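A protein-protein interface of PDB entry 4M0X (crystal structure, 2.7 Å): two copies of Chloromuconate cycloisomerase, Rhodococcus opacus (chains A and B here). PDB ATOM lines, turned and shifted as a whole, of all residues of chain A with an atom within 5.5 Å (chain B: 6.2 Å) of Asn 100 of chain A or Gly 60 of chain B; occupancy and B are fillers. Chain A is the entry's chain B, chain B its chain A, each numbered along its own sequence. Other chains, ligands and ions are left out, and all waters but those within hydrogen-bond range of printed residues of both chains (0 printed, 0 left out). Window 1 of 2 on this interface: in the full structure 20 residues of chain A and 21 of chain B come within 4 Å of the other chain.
Among the printed residues, pairs that only touch across the chains: Ile 69 of chain A with Thr 65 of chain B, Val 97 of chain A with Pro 56 of chain B, Phe 98 of chain A with Trp 57 of chain B, Phe 98 of chain A with Trp 58 of chain B, Phe 98 of chain A with Gly 59 of chain B and Phe 98 of chain A with Gly 60 of chain B.
Of the 10 printed residues of chain B, 6 touch a printed residue of chain A.
Along chain B the printed residues that touch a printed residue of chain A span positions 56 to 65.
Hydrophobic or aromatic side chains of chain A within 4 Å of the printed part of chain B: Ile 69, Val 97 and Phe 98.
Among the printed residues, 8 pairs touch across the chains.
Positions printed for both chains: 61 and 100.
Of the 8 pairs that touch across the chains among the printed residues, none has its exchanged pair printed and touching as well.
The backbone carbonyl oxygen of Pro 56 of chain B is in hydrogen-bond range of the backbone NH of Phe 98 of chain A, 2.9 Å away.
The backbone carbonyl oxygen (O) of Gly 60 of chain B lies within hydrogen-bond range of the side-chain amide nitrogen (ND2) of Asn 100 of chain A (2.9 Å).
N of Thr 65 of chain B is in hydrogen-bond range of OG of Ser 62 of chain B (3.1 Å).
The backbone carbonyl oxygen (O) of Ile 69 of chain A sits at hydrogen-bond distance from the backbone NH (N) of Leu 74 of chain A, 2.8 Å away.
O of Val 97 of chain A is in hydrogen-bond range of NZ of Lys 104 of chain A (2.9 Å).
The side-chain amide nitrogen of Asn 100 of chain A is in hydrogen-bond range of the backbone carbonyl oxygen of Phe 98 of chain A, 3.0 Å away.
Of the printed residues of chain B, Val 97 of chain A touches Pro 56 (3.7 Å).
Printed residues of chain B within 4 Å of Phe 98 of chain A: Pro 56, Trp 57, Trp 58, Gly 59 and Gly 60.
Asn 100 of chain A touches just one residue of chain B: Gly 60 (2.9 Å).
Val 102 of chain A touches none of the printed residues of chain B.
Printed residues of chain A within 4 Å of Pro 56 of chain B: Val 97 and Phe 98.
Of the printed residues of chain A, Gly 59 of chain B touches Phe 98 (3.8 Å).
Ser 62 of chain B touches none of the printed residues of chain A.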
ATOM      1  N   GLU A  61      -0.320  16.033  14.924  1.00  0.00           N
ATOM      2  CA  GLU A  61      -0.141  15.944  13.478  1.00  0.00           C
ATOM      3  C   GLU A  61       0.977  16.839  13.013  1.00  0.00           C
ATOM      4  O   GLU A  61       1.242  17.889  13.598  1.00  0.00           O
ATOM      5  CB  GLU A  61      -1.457  16.212  12.721  1.00  0.00           C
ATOM      6  CG  GLU A  61      -2.401  15.016  12.729  1.00  0.00           C
ATOM      7  CD  GLU A  61      -3.796  15.304  12.187  1.00  0.00           C
ATOM      8  OE1 GLU A  61      -4.050  14.921  11.020  1.00  0.00           O
ATOM      9  OE2 GLU A  61      -4.645  15.899  12.915  1.00  0.00           O
ATOM     10  N   ILE A  69       0.303   9.629   5.750  1.00  0.00           N
ATOM     11  CA  ILE A  69      -1.046   9.130   5.997  1.00  0.00           C
ATOM     12  C   ILE A  69      -1.857   9.230   4.720  1.00  0.00           C
ATOM     13  O   ILE A  69      -2.458   8.248   4.264  1.00  0.00           O
ATOM     14  CB  ILE A  69      -1.711   9.843   7.194  1.00  0.00           C
ATOM     15  CG1 ILE A  69      -1.024   9.441   8.527  1.00  0.00           C
ATOM     16  CG2 ILE A  69      -3.201   9.543   7.250  1.00  0.00           C
ATOM     17  CD1 ILE A  69      -1.146   7.976   8.923  1.00  0.00           C
ATOM     18  N   LEU A  74      -4.589   6.778   3.139  1.00  0.00           N
ATOM     19  CA  LEU A  74      -5.856   7.368   2.688  1.00  0.00           C
ATOM     20  C   LEU A  74      -6.107   7.315   1.177  1.00  0.00           C
ATOM     21  O   LEU A  74      -7.265   7.396   0.739  1.00  0.00           O
ATOM     22  CB  LEU A  74      -6.007   8.798   3.203  1.00  0.00           C
ATOM     23  CG  LEU A  74      -6.035   8.958   4.714  1.00  0.00           C
ATOM     24  CD1 LEU A  74      -6.015  10.435   5.069  1.00  0.00           C
ATOM     25  CD2 LEU A  74      -7.267   8.291   5.268  1.00  0.00           C
ATOM     26  N   VAL A  97      -8.494   4.842   8.901  1.00  0.00           N
ATOM     27  CA  VAL A  97      -7.635   5.639   9.749  1.00  0.00           C
ATOM     28  C   VAL A  97      -8.459   6.234  10.843  1.00  0.00           C
ATOM     29  O   VAL A  97      -9.334   7.045  10.571  1.00  0.00           O
ATOM     30  CB  VAL A  97      -6.995   6.808   8.990  1.00  0.00           C
ATOM     31  CG1 VAL A  97      -6.224   7.701   9.950  1.00  0.00           C
ATOM     32  CG2 VAL A  97      -6.048   6.284   7.935  1.00  0.00           C
ATOM     33  N   PHE A  98      -8.191   5.837  12.076  1.00  0.00           N
ATOM     34  CA  PHE A  98      -8.659   6.642  13.179  1.00  0.00           C
ATOM     35  C   PHE A  98      -7.890   7.989  13.285  1.00  0.00           C
ATOM     36  O   PHE A  98      -6.698   8.078  12.943  1.00  0.00           O
ATOM     37  CB  PHE A  98      -8.657   5.870  14.508  1.00  0.00           C
ATOM     38  CG  PHE A  98      -9.200   6.673  15.663  1.00  0.00           C
ATOM     39  CD1 PHE A  98     -10.557   6.779  15.873  1.00  0.00           C
ATOM     40  CD2 PHE A  98      -8.345   7.355  16.525  1.00  0.00           C
ATOM     41  CE1 PHE A  98     -11.048   7.530  16.929  1.00  0.00           C
ATOM     42  CE2 PHE A  98      -8.833   8.109  17.585  1.00  0.00           C
ATOM     43  CZ  PHE A  98     -10.187   8.199  17.788  1.00  0.00           C
ATOM     44  N   GLY A  99      -8.597   9.018  13.765  1.00  0.00           N
ATOM     45  CA  GLY A  99      -8.045  10.333  13.955  1.00  0.00           C
ATOM     46  C   GLY A  99      -7.527  10.938  12.670  1.00  0.00           C
ATOM     47  O   GLY A  99      -8.184  10.841  11.616  1.00  0.00           O
ATOM     48  N   ASN A 100      -6.347  11.554  12.749  1.00  0.00           N
ATOM     49  CA  ASN A 100      -5.731  12.238  11.603  1.00  0.00           C
ATOM     50  C   ASN A 100      -6.711  13.133  10.854  1.00  0.00           C
ATOM     51  O   ASN A 100      -6.858  13.051   9.630  1.00  0.00           O
ATOM     52  CB  ASN A 100      -5.017  11.247  10.663  1.00  0.00           C
ATOM     53  CG  ASN A 100      -3.885  10.506  11.362  1.00  0.00           C
ATOM     54  OD1 ASN A 100      -2.756  10.982  11.428  1.00  0.00           O
ATOM     55  ND2 ASN A 100      -4.202   9.345  11.923  1.00  0.00           N
ATOM     56  N   SER A 101      -7.375  14.003  11.610  1.00  0.00           N
ATOM     57  CA  SER A 101      -8.334  14.967  11.050  1.00  0.00           C
ATOM     58  C   SER A 101      -7.757  15.962  10.022  1.00  0.00           C
ATOM     59  O   SER A 101      -8.407  16.225   9.010  1.00  0.00           O
ATOM     60  CB  SER A 101      -9.052  15.711  12.173  1.00  0.00           C
ATOM     61  OG  SER A 101      -9.772  14.789  12.961  1.00  0.00           O
ATOM     62  N   VAL A 102      -6.566  16.516  10.284  1.00  0.00           N
ATOM     63  CA  VAL A 102      -5.970  17.521   9.386  1.00  0.00           C
ATOM     64  C   VAL A 102      -5.630  16.913   8.012  1.00  0.00           C
ATOM     65  O   VAL A 102      -5.862  17.529   6.956  1.00  0.00           O
ATOM     66  CB  VAL A 102      -4.730  18.204  10.032  1.00  0.00           C
ATOM     67  CG1 VAL A 102      -4.060  19.176   9.066  1.00  0.00           C
ATOM     68  CG2 VAL A 102      -5.107  18.917  11.347  1.00  0.00           C
ATOM     69  N   ALA A 103      -5.092  15.701   8.014  1.00  0.00           N
ATOM     70  CA  ALA A 103      -4.893  14.964   6.757  1.00  0.00           C
ATOM     71  C   ALA A 103      -6.231  14.770   6.071  1.00  0.00           C
ATOM     72  O   ALA A 103      -6.392  15.145   4.911  1.00  0.00           O
ATOM     73  CB  ALA A 103      -4.219  13.627   7.003  1.00  0.00           C
ATOM     74  N   LYS A 104      -7.203  14.220   6.805  1.00  0.00           N
ATOM     75  CA  LYS A 104      -8.531  13.998   6.253  1.00  0.00           C
ATOM     76  C   LYS A 104      -9.122  15.268   5.683  1.00  0.00           C
ATOM     77  O   LYS A 104      -9.615  15.245   4.560  1.00  0.00           O
ATOM     78  CB  LYS A 104      -9.464  13.406   7.297  1.00  0.00           C
ATOM     79  CG  LYS A 104      -9.279  11.904   7.503  1.00  0.00           C
ATOM     80  CD  LYS A 104      -9.767  11.459   8.885  1.00  0.00           C
ATOM     81  CE  LYS A 104      -9.555   9.984   9.115  1.00  0.00           C
ATOM     82  NZ  LYS A 104     -10.625   9.552  10.027  1.00  0.00           N
ATOM     83  N   ALA A 105      -9.068  16.364   6.440  1.00  0.00           N
ATOM     84  CA  ALA A 105      -9.688  17.613   6.028  1.00  0.00           C
ATOM     85  C   ALA A 105      -9.108  18.072   4.697  1.00  0.00           C
ATOM     86  O   ALA A 105      -9.842  18.562   3.834  1.00  0.00           O
ATOM     87  CB  ALA A 105      -9.490  18.688   7.065  1.00  0.00           C
ATOM     88  N   GLY B  55      -2.050  -1.203  11.628  1.00  0.00           N
ATOM     89  CA  GLY B  55      -2.149   0.088  10.929  1.00  0.00           C
ATOM     90  C   GLY B  55      -2.977   1.106  11.705  1.00  0.00           C
ATOM     91  O   GLY B  55      -3.376   0.846  12.846  1.00  0.00           O
ATOM     92  N   PRO B  56      -3.260   2.264  11.093  1.00  0.00           N
ATOM     93  CA  PRO B  56      -3.856   3.344  11.856  1.00  0.00           C
ATOM     94  C   PRO B  56      -5.365   3.247  12.065  1.00  0.00           C
ATOM     95  O   PRO B  56      -5.952   4.122  12.689  1.00  0.00           O
ATOM     96  CB  PRO B  56      -3.462   4.590  11.066  1.00  0.00           C
ATOM     97  CG  PRO B  56      -3.374   4.102   9.677  1.00  0.00           C
ATOM     98  CD  PRO B  56      -2.842   2.700   9.755  1.00  0.00           C
ATOM     99  N   TRP B  57      -5.982   2.173  11.594  1.00  0.00           N
ATOM    100  CA  TRP B  57      -7.426   1.991  11.771  1.00  0.00           C
ATOM    101  C   TRP B  57      -7.852   2.085  13.247  1.00  0.00           C
ATOM    102  O   TRP B  57      -8.893   2.670  13.551  1.00  0.00           O
ATOM    103  CB  TRP B  57      -7.889   0.667  11.135  1.00  0.00           C
ATOM    104  CG  TRP B  57      -7.555  -0.555  11.978  1.00  0.00           C
ATOM    105  CD1 TRP B  57      -6.395  -1.289  11.942  1.00  0.00           C
ATOM    106  CD2 TRP B  57      -8.365  -1.144  13.016  1.00  0.00           C
ATOM    107  NE1 TRP B  57      -6.442  -2.308  12.872  1.00  0.00           N
ATOM    108  CE2 TRP B  57      -7.633  -2.244  13.546  1.00  0.00           C
ATOM    109  CE3 TRP B  57      -9.634  -0.848  13.554  1.00  0.00           C
ATOM    110  CZ2 TRP B  57      -8.131  -3.052  14.587  1.00  0.00           C
ATOM    111  CZ3 TRP B  57     -10.133  -1.659  14.579  1.00  0.00           C
ATOM    112  CH2 TRP B  57      -9.373  -2.747  15.086  1.00  0.00           C
ATOM    113  N   TRP B  58      -7.037   1.544  14.157  1.00  0.00           N
ATOM    114  CA  TRP B  58      -7.414   1.437  15.561  1.00  0.00           C
ATOM    115  C   TRP B  58      -7.184   2.741  16.314  1.00  0.00           C
ATOM    116  O   TRP B  58      -8.077   3.222  17.003  1.00  0.00           O
ATOM    117  CB  TRP B  58      -6.624   0.308  16.209  1.00  0.00           C
ATOM    118  CG  TRP B  58      -7.090  -0.172  17.598  1.00  0.00           C
ATOM    119  CD1 TRP B  58      -7.710  -1.354  17.885  1.00  0.00           C
ATOM    120  CD2 TRP B  58      -6.895   0.493  18.867  1.00  0.00           C
ATOM    121  NE1 TRP B  58      -7.930  -1.461  19.237  1.00  0.00           N
ATOM    122  CE2 TRP B  58      -7.459  -0.338  19.862  1.00  0.00           C
ATOM    123  CE3 TRP B  58      -6.313   1.722  19.256  1.00  0.00           C
ATOM    124  CZ2 TRP B  58      -7.461   0.014  21.223  1.00  0.00           C
ATOM    125  CZ3 TRP B  58      -6.321   2.083  20.622  1.00  0.00           C
ATOM    126  CH2 TRP B  58      -6.887   1.232  21.581  1.00  0.00           C
ATOM    127  N   GLY B  59      -5.980   3.297  16.192  1.00  0.00           N
ATOM    128  CA  GLY B  59      -5.554   4.419  17.038  1.00  0.00           C
ATOM    129  C   GLY B  59      -4.948   5.607  16.298  1.00  0.00           C
ATOM    130  O   GLY B  59      -4.566   6.599  16.931  1.00  0.00           O
ATOM    131  N   GLY B  60      -4.862   5.525  14.966  1.00  0.00           N
ATOM    132  CA  GLY B  60      -4.366   6.646  14.154  1.00  0.00           C
ATOM    133  C   GLY B  60      -2.842   6.749  14.040  1.00  0.00           C
ATOM    134  O   GLY B  60      -2.295   7.720  13.471  1.00  0.00           O
ATOM    135  N   GLU B  61      -2.155   5.752  14.591  1.00  0.00           N
ATOM    136  CA  GLU B  61      -0.709   5.702  14.518  1.00  0.00           C
ATOM    137  C   GLU B  61      -0.367   4.598  13.533  1.00  0.00           C
ATOM    138  O   GLU B  61      -1.151   3.650  13.386  1.00  0.00           O
ATOM    139  CB  GLU B  61      -0.100   5.458  15.910  1.00  0.00           C
ATOM    140  CG  GLU B  61      -0.488   6.532  16.929  1.00  0.00           C
ATOM    141  CD  GLU B  61       0.474   6.683  18.112  1.00  0.00           C
ATOM    142  OE1 GLU B  61       1.669   7.020  17.888  1.00  0.00           O
ATOM    143  OE2 GLU B  61       0.029   6.511  19.278  1.00  0.00           O
ATOM    144  N   SER B  62       0.761   4.761  12.828  1.00  0.00           N
ATOM    145  CA  SER B  62       1.319   3.739  11.923  1.00  0.00           C
ATOM    146  C   SER B  62       2.823   3.584  12.126  1.00  0.00           C
ATOM    147  O   SER B  62       3.496   4.541  12.517  1.00  0.00           O
ATOM    148  CB  SER B  62       1.069   4.117  10.472  1.00  0.00           C
ATOM    149  OG  SER B  62       1.937   5.158  10.045  1.00  0.00           O
ATOM    150  N   THR B  65       4.680   6.514  10.422  1.00  0.00           N
ATOM    151  CA  THR B  65       4.588   7.830  11.050  1.00  0.00           C
ATOM    152  C   THR B  65       5.154   7.825  12.449  1.00  0.00           C
ATOM    153  O   THR B  65       5.604   8.874  12.948  1.00  0.00           O
ATOM    154  CB  THR B  65       3.157   8.355  11.119  1.00  0.00           C
ATOM    155  OG1 THR B  65       2.393   7.531  12.013  1.00  0.00           O
ATOM    156  CG2 THR B  65       2.538   8.365   9.752  1.00  0.00           C
ATOM    157  N   ASN B 100      -0.063  10.601  19.962  1.00  0.00           N
ATOM    158  CA  ASN B 100       1.055   9.755  19.558  1.00  0.00           C
ATOM    159  C   ASN B 100       1.586   8.951  20.727  1.00  0.00           C
ATOM    160  O   ASN B 100       2.768   9.029  21.070  1.00  0.00           O
ATOM    161  CB  ASN B 100       2.162  10.569  18.871  1.00  0.00           C
ATOM    162  CG  ASN B 100       1.725  11.114  17.508  1.00  0.00           C
ATOM    163  OD1 ASN B 100       1.994  10.526  16.462  1.00  0.00           O
ATOM    164  ND2 ASN B 100       1.040  12.227  17.520  1.00  0.00           N
